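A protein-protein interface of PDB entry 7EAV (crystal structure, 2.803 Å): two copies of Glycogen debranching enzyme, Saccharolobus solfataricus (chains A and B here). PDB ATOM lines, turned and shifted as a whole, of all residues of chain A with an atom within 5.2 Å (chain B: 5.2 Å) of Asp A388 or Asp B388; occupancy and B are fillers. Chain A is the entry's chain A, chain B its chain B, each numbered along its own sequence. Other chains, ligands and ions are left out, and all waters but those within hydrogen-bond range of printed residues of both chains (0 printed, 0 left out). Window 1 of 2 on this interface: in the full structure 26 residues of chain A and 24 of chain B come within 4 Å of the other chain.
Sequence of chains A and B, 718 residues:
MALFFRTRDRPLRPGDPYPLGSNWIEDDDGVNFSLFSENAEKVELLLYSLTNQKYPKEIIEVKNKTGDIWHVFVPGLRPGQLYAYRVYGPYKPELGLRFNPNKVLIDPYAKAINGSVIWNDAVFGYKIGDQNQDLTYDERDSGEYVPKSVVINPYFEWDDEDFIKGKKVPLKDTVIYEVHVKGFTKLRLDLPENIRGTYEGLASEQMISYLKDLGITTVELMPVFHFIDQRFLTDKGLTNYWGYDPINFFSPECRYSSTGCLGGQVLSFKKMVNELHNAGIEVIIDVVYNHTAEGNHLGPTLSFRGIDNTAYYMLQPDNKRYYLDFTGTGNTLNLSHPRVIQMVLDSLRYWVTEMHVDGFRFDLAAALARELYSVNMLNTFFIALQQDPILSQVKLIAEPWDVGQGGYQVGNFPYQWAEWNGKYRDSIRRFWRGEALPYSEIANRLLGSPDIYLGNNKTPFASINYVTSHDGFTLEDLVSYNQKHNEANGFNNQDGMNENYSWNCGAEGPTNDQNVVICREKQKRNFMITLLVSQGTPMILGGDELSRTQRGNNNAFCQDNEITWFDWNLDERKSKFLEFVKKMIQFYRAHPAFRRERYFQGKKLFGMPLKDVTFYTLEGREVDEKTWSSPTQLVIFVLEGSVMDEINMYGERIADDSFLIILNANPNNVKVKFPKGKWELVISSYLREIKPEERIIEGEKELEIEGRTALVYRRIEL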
ATOM      1  N   ARG A 349       9.067 -19.663 -14.083  1.00  0.00           N
ATOM      2  CA  ARG A 349       8.307 -19.007 -15.140  1.00  0.00           C
ATOM      3  C   ARG A 349       6.851 -18.819 -14.737  1.00  0.00           C
ATOM      4  O   ARG A 349       6.247 -17.783 -15.043  1.00  0.00           O
ATOM      5  CB  ARG A 349       8.404 -19.811 -16.432  1.00  0.00           C
ATOM      6  CG  ARG A 349       9.725 -19.663 -17.151  1.00  0.00           C
ATOM      7  CD  ARG A 349       9.691 -20.390 -18.476  1.00  0.00           C
ATOM      8  NE  ARG A 349       9.727 -21.839 -18.303  1.00  0.00           N
ATOM      9  CZ  ARG A 349      10.820 -22.581 -18.455  1.00  0.00           C
ATOM     10  NH1 ARG A 349      11.970 -22.010 -18.785  1.00  0.00           N
ATOM     11  NH2 ARG A 349      10.762 -23.894 -18.277  1.00  0.00           N
ATOM     12  N   ILE A 383      22.866 -22.306 -16.035  1.00  0.00           N
ATOM     13  CA  ILE A 383      23.032 -21.885 -17.424  1.00  0.00           C
ATOM     14  C   ILE A 383      21.674 -21.673 -18.082  1.00  0.00           C
ATOM     15  O   ILE A 383      21.433 -20.651 -18.737  1.00  0.00           O
ATOM     16  CB  ILE A 383      23.878 -22.913 -18.198  1.00  0.00           C
ATOM     17  CG1 ILE A 383      25.341 -22.846 -17.757  1.00  0.00           C
ATOM     18  CG2 ILE A 383      23.756 -22.684 -19.698  1.00  0.00           C
ATOM     19  CD1 ILE A 383      26.265 -23.737 -18.564  1.00  0.00           C
ATOM     20  N   ALA A 384      20.764 -22.637 -17.913  1.00  0.00           N
ATOM     21  CA  ALA A 384      19.434 -22.511 -18.499  1.00  0.00           C
ATOM     22  C   ALA A 384      18.699 -21.297 -17.945  1.00  0.00           C
ATOM     23  O   ALA A 384      17.943 -20.634 -18.666  1.00  0.00           O
ATOM     24  CB  ALA A 384      18.629 -23.786 -18.253  1.00  0.00           C
ATOM     25  N   LEU A 385      18.911 -20.989 -16.664  1.00  0.00           N
ATOM     26  CA  LEU A 385      18.306 -19.795 -16.082  1.00  0.00           C
ATOM     27  C   LEU A 385      18.866 -18.530 -16.718  1.00  0.00           C
ATOM     28  O   LEU A 385      18.136 -17.553 -16.925  1.00  0.00           O
ATOM     29  CB  LEU A 385      18.528 -19.789 -14.569  1.00  0.00           C
ATOM     30  CG  LEU A 385      18.133 -18.537 -13.784  1.00  0.00           C
ATOM     31  CD1 LEU A 385      16.686 -18.166 -14.041  1.00  0.00           C
ATOM     32  CD2 LEU A 385      18.367 -18.754 -12.301  1.00  0.00           C
ATOM     33  N   GLN A 386      20.161 -18.532 -17.047  1.00  0.00           N
ATOM     34  CA  GLN A 386      20.777 -17.346 -17.633  1.00  0.00           C
ATOM     35  C   GLN A 386      20.306 -17.110 -19.064  1.00  0.00           C
ATOM     36  O   GLN A 386      20.241 -15.957 -19.508  1.00  0.00           O
ATOM     37  CB  GLN A 386      22.301 -17.475 -17.589  1.00  0.00           C
ATOM     38  CG  GLN A 386      23.046 -16.218 -18.011  1.00  0.00           C
ATOM     39  CD  GLN A 386      24.537 -16.447 -18.168  1.00  0.00           C
ATOM     40  OE1 GLN A 386      25.326 -16.098 -17.292  1.00  0.00           O
ATOM     41  NE2 GLN A 386      24.928 -17.038 -19.292  1.00  0.00           N
ATOM     42  N   GLN A 387      19.965 -18.172 -19.793  1.00  0.00           N
ATOM     43  CA  GLN A 387      19.609 -18.046 -21.200  1.00  0.00           C
ATOM     44  C   GLN A 387      18.123 -17.812 -21.438  1.00  0.00           C
ATOM     45  O   GLN A 387      17.755 -17.336 -22.518  1.00  0.00           O
ATOM     46  CB  GLN A 387      20.041 -19.299 -21.972  1.00  0.00           C
ATOM     47  CG  GLN A 387      19.308 -20.577 -21.567  1.00  0.00           C
ATOM     48  CD  GLN A 387      18.017 -20.794 -22.341  1.00  0.00           C
ATOM     49  OE1 GLN A 387      17.965 -20.588 -23.553  1.00  0.00           O
ATOM     50  NE2 GLN A 387      16.968 -21.203 -21.637  1.00  0.00           N
ATOM     51  N   ASP A 388      17.270 -18.136 -20.471  1.00  0.00           N
ATOM     52  CA  ASP A 388      15.830 -18.163 -20.718  1.00  0.00           C
ATOM     53  C   ASP A 388      15.310 -16.769 -21.054  1.00  0.00           C
ATOM     54  O   ASP A 388      15.638 -15.807 -20.353  1.00  0.00           O
ATOM     55  CB  ASP A 388      15.089 -18.714 -19.506  1.00  0.00           C
ATOM     56  CG  ASP A 388      13.613 -18.915 -19.775  1.00  0.00           C
ATOM     57  OD1 ASP A 388      13.280 -19.712 -20.678  1.00  0.00           O
ATOM     58  OD2 ASP A 388      12.788 -18.274 -19.092  1.00  0.00           O
ATOM     59  N   PRO A 389      14.497 -16.622 -22.105  1.00  0.00           N
ATOM     60  CA  PRO A 389      14.024 -15.277 -22.481  1.00  0.00           C
ATOM     61  C   PRO A 389      13.187 -14.588 -21.415  1.00  0.00           C
ATOM     62  O   PRO A 389      13.281 -13.364 -21.264  1.00  0.00           O
ATOM     63  CB  PRO A 389      13.210 -15.544 -23.755  1.00  0.00           C
ATOM     64  CG  PRO A 389      13.781 -16.803 -24.312  1.00  0.00           C
ATOM     65  CD  PRO A 389      14.167 -17.634 -23.123  1.00  0.00           C
ATOM     66  N   ILE A 390      12.366 -15.331 -20.671  1.00  0.00           N
ATOM     67  CA  ILE A 390      11.492 -14.696 -19.685  1.00  0.00           C
ATOM     68  C   ILE A 390      12.247 -14.416 -18.394  1.00  0.00           C
ATOM     69  O   ILE A 390      12.243 -13.288 -17.886  1.00  0.00           O
ATOM     70  CB  ILE A 390      10.245 -15.564 -19.431  1.00  0.00           C
ATOM     71  CG1 ILE A 390       9.268 -15.453 -20.602  1.00  0.00           C
ATOM     72  CG2 ILE A 390       9.562 -15.149 -18.137  1.00  0.00           C
ATOM     73  CD1 ILE A 390       8.067 -16.367 -20.477  1.00  0.00           C
ATOM     74  N   LEU A 391      12.906 -15.436 -17.841  1.00  0.00           N
ATOM     75  CA  LEU A 391      13.625 -15.267 -16.583  1.00  0.00           C
ATOM     76  C   LEU A 391      14.812 -14.323 -16.718  1.00  0.00           C
ATOM     77  O   LEU A 391      15.303 -13.816 -15.704  1.00  0.00           O
ATOM     78  CB  LEU A 391      14.081 -16.631 -16.065  1.00  0.00           C
ATOM     79  CG  LEU A 391      12.936 -17.615 -15.803  1.00  0.00           C
ATOM     80  CD1 LEU A 391      13.446 -18.981 -15.362  1.00  0.00           C
ATOM     81  CD2 LEU A 391      11.957 -17.053 -14.780  1.00  0.00           C
ATOM     82  N   SER A 392      15.272 -14.065 -17.941  1.00  0.00           N
ATOM     83  CA  SER A 392      16.344 -13.100 -18.150  1.00  0.00           C
ATOM     84  C   SER A 392      15.965 -11.686 -17.732  1.00  0.00           C
ATOM     85  O   SER A 392      16.861 -10.855 -17.558  1.00  0.00           O
ATOM     86  CB  SER A 392      16.766 -13.086 -19.614  1.00  0.00           C
ATOM     87  OG  SER A 392      15.627 -13.079 -20.455  1.00  0.00           O
ATOM     88  N   ARG B 349      14.999 -20.571 -31.091  1.00  0.00           N
ATOM     89  CA  ARG B 349      13.793 -19.825 -30.752  1.00  0.00           C
ATOM     90  C   ARG B 349      13.498 -18.752 -31.791  1.00  0.00           C
ATOM     91  O   ARG B 349      12.331 -18.476 -32.091  1.00  0.00           O
ATOM     92  CB  ARG B 349      13.930 -19.198 -29.365  1.00  0.00           C
ATOM     93  CG  ARG B 349      13.704 -20.164 -28.214  1.00  0.00           C
ATOM     94  CD  ARG B 349      13.682 -19.430 -26.883  1.00  0.00           C
ATOM     95  NE  ARG B 349      15.020 -19.028 -26.459  1.00  0.00           N
ATOM     96  CZ  ARG B 349      15.820 -19.773 -25.703  1.00  0.00           C
ATOM     97  NH1 ARG B 349      15.419 -20.967 -25.288  1.00  0.00           N
ATOM     98  NH2 ARG B 349      17.022 -19.327 -25.364  1.00  0.00           N
ATOM     99  N   ILE B 383      19.308 -30.618 -22.341  1.00  0.00           N
ATOM    100  CA  ILE B 383      18.386 -30.447 -21.218  1.00  0.00           C
ATOM    101  C   ILE B 383      17.635 -29.127 -21.342  1.00  0.00           C
ATOM    102  O   ILE B 383      16.403 -29.081 -21.232  1.00  0.00           O
ATOM    103  CB  ILE B 383      19.145 -30.534 -19.882  1.00  0.00           C
ATOM    104  CG1 ILE B 383      19.745 -31.927 -19.690  1.00  0.00           C
ATOM    105  CG2 ILE B 383      18.225 -30.190 -18.723  1.00  0.00           C
ATOM    106  CD1 ILE B 383      20.665 -32.027 -18.492  1.00  0.00           C
ATOM    107  N   ALA B 384      18.368 -28.035 -21.568  1.00  0.00           N
ATOM    108  CA  ALA B 384      17.730 -26.728 -21.699  1.00  0.00           C
ATOM    109  C   ALA B 384      16.770 -26.695 -22.881  1.00  0.00           C
ATOM    110  O   ALA B 384      15.714 -26.057 -22.815  1.00  0.00           O
ATOM    111  CB  ALA B 384      18.791 -25.637 -21.833  1.00  0.00           C
ATOM    112  N   LEU B 385      17.121 -27.377 -23.975  1.00  0.00           N
ATOM    113  CA  LEU B 385      16.200 -27.489 -25.102  1.00  0.00           C
ATOM    114  C   LEU B 385      14.937 -28.243 -24.705  1.00  0.00           C
ATOM    115  O   LEU B 385      13.829 -27.871 -25.106  1.00  0.00           O
ATOM    116  CB  LEU B 385      16.893 -28.180 -26.278  1.00  0.00           C
ATOM    117  CG  LEU B 385      16.055 -28.505 -27.519  1.00  0.00           C
ATOM    118  CD1 LEU B 385      15.677 -27.247 -28.283  1.00  0.00           C
ATOM    119  CD2 LEU B 385      16.798 -29.480 -28.423  1.00  0.00           C
ATOM    120  N   GLN B 386      15.087 -29.300 -23.905  1.00  0.00           N
ATOM    121  CA  GLN B 386      13.939 -30.104 -23.502  1.00  0.00           C
ATOM    122  C   GLN B 386      12.989 -29.316 -22.606  1.00  0.00           C
ATOM    123  O   GLN B 386      11.766 -29.465 -22.707  1.00  0.00           O
ATOM    124  CB  GLN B 386      14.422 -31.370 -22.794  1.00  0.00           C
ATOM    125  CG  GLN B 386      13.346 -32.407 -22.535  1.00  0.00           C
ATOM    126  CD  GLN B 386      13.814 -33.494 -21.586  1.00  0.00           C
ATOM    127  OE1 GLN B 386      14.263 -34.557 -22.013  1.00  0.00           O
ATOM    128  NE2 GLN B 386      13.715 -33.230 -20.288  1.00  0.00           N
ATOM    129  N   GLN B 387      13.530 -28.466 -21.731  1.00  0.00           N
ATOM    130  CA  GLN B 387      12.701 -27.740 -20.777  1.00  0.00           C
ATOM    131  C   GLN B 387      12.105 -26.462 -21.350  1.00  0.00           C
ATOM    132  O   GLN B 387      11.178 -25.909 -20.747  1.00  0.00           O
ATOM    133  CB  GLN B 387      13.515 -27.398 -19.525  1.00  0.00           C
ATOM    134  CG  GLN B 387      14.653 -26.401 -19.756  1.00  0.00           C
ATOM    135  CD  GLN B 387      14.197 -24.951 -19.718  1.00  0.00           C
ATOM    136  OE1 GLN B 387      13.368 -24.568 -18.892  1.00  0.00           O
ATOM    137  NE2 GLN B 387      14.732 -24.139 -20.623  1.00  0.00           N
ATOM    138  N   ASP B 388      12.616 -25.978 -22.478  1.00  0.00           N
ATOM    139  CA  ASP B 388      12.241 -24.655 -22.953  1.00  0.00           C
ATOM    140  C   ASP B 388      10.755 -24.615 -23.301  1.00  0.00           C
ATOM    141  O   ASP B 388      10.225 -25.569 -23.879  1.00  0.00           O
ATOM    142  CB  ASP B 388      13.080 -24.266 -24.171  1.00  0.00           C
ATOM    143  CG  ASP B 388      12.871 -22.825 -24.581  1.00  0.00           C
ATOM    144  OD1 ASP B 388      13.293 -21.920 -23.828  1.00  0.00           O
ATOM    145  OD2 ASP B 388      12.278 -22.596 -25.654  1.00  0.00           O
ATOM    146  N   PRO B 389      10.052 -23.531 -22.955  1.00  0.00           N
ATOM    147  CA  PRO B 389       8.597 -23.497 -23.193  1.00  0.00           C
ATOM    148  C   PRO B 389       8.199 -23.618 -24.654  1.00  0.00           C
ATOM    149  O   PRO B 389       7.266 -24.366 -24.972  1.00  0.00           O
ATOM    150  CB  PRO B 389       8.184 -22.138 -22.611  1.00  0.00           C
ATOM    151  CG  PRO B 389       9.232 -21.814 -21.621  1.00  0.00           C
ATOM    152  CD  PRO B 389      10.510 -22.401 -22.132  1.00  0.00           C
ATOM    153  N   ILE B 390       8.868 -22.905 -25.556  1.00  0.00           N
ATOM    154  CA  ILE B 390       8.436 -22.904 -26.950  1.00  0.00           C
ATOM    155  C   ILE B 390       9.117 -24.011 -27.749  1.00  0.00           C
ATOM    156  O   ILE B 390       8.477 -24.673 -28.569  1.00  0.00           O
ATOM    157  CB  ILE B 390       8.671 -21.513 -27.576  1.00  0.00           C
ATOM    158  CG1 ILE B 390       8.216 -21.498 -29.037  1.00  0.00           C
ATOM    159  CG2 ILE B 390      10.128 -21.112 -27.486  1.00  0.00           C
ATOM    160  CD1 ILE B 390       6.718 -21.623 -29.227  1.00  0.00           C
ATOM    161  N   LEU B 391      10.409 -24.260 -27.517  1.00  0.00           N
ATOM    162  CA  LEU B 391      11.104 -25.292 -28.280  1.00  0.00           C
ATOM    163  C   LEU B 391      10.637 -26.696 -27.915  1.00  0.00           C
ATOM    164  O   LEU B 391      10.875 -27.635 -28.682  1.00  0.00           O
ATOM    165  CB  LEU B 391      12.611 -25.161 -28.082  1.00  0.00           C
ATOM    166  CG  LEU B 391      13.183 -23.861 -28.650  1.00  0.00           C
ATOM    167  CD1 LEU B 391      14.680 -23.781 -28.437  1.00  0.00           C
ATOM    168  CD2 LEU B 391      12.847 -23.728 -30.129  1.00  0.00           C
ATOM    169  N   SER B 392       9.965 -26.860 -26.775  1.00  0.00           N
ATOM    170  CA  SER B 392       9.359 -28.136 -26.420  1.00  0.00           C
ATOM    171  C   SER B 392       8.165 -28.500 -27.296  1.00  0.00           C
ATOM    172  O   SER B 392       7.608 -29.589 -27.118  1.00  0.00           O
ATOM    173  CB  SER B 392       8.908 -28.112 -24.960  1.00  0.00           C
ATOM    174  OG  SER B 392       8.071 -26.994 -24.714  1.00  0.00           O
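NH2 of Arg A349 is in hydrogen-bond range of OE1 of Gln B387, 2.8 Å away.
The side-chain amide oxygen of Gln A387 lies within hydrogen-bond range of the guanidinium group of Arg B349 (2.4 Å).
The backbone NH (N) of Ile A390 lies close to the side-chain carboxylate (OD2) of Asp A388, 3.4 Å away.
The backbone carbonyl oxygen (O) of Asp A388 lies within hydrogen-bond range of the side-chain hydroxyl (OG) of Ser A392 (2.7 Å).
The side-chain hydroxyl (OG) of Ser A392 sits at hydrogen-bond distance from the backbone carbonyl oxygen (O) of Pro A389 (2.5 Å).
O of Ala B384 is in hydrogen-bond range of NE2 of Gln B387, at 3.1 Å.
The backbone NH of Ile B390 lies close to the side-chain carboxylate of Asp B388, 3.4 Å away.
The side-chain hydroxyl (OG) of Ser B392 sits at hydrogen-bond distance from the backbone carbonyl oxygen (O) of Asp B388 (2.7 Å).
Among the printed residues, merely in contact across the chains: Pro A389 with Arg B349 (3.3 Å), Arg A349 with Pro B389 (3.4 Å), Gln A387 with Gln B387 (3.8 Å) and Asp A388 with Asp B388 (3.8 Å).
Of the printed residues of chain B, Arg A349 touches Gln B387 and Pro B389.
Ala A384 touches none of the printed residues of chain B.
Of the printed residues of chain B, Gln A387 touches Arg B349 (2.4 Å) and Gln B387 (3.8 Å).
Of the printed residues of chain B, Pro A389 touches Arg B349.
Of the printed residues of chain A, Gln B387 touches Arg A349 (2.8 Å) and Gln A387 (3.8 Å).
Of chain A, only Asp A388 (3.8 Å) comes within 4 Å of Asp B388.
Printed residues of chain A within 4 Å of Pro B389: Arg A349 (3.4 Å).
The nearest residue of chain B that does not touch Asp A388 is Pro B389 (4.1 Å).
The nearest printed residue of chain A that does not touch Pro B389 is Asp A388 (4.1 Å).
Of the 11 printed residues of chain A, 4 touch a printed residue of chain B.
Printed residues of chain A that touch a printed residue of chain B: Arg A349, Gln A387, Asp A388 and Pro A389.
Among the printed residues, no Asp or Glu carboxylate lies within 4 Å of a Lys or Arg side-chain nitrogen of the other chain.
Arg A349 touches Gln B387, and with the chains exchanged Gln A387 touches Arg B349.
Arg A349 touches Pro B389, and with the chains exchanged Pro A389 touches Arg B349.
Gln A387 touches its own counterpart, Gln B387.
Asp A388 touches its own counterpart, Asp B388.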
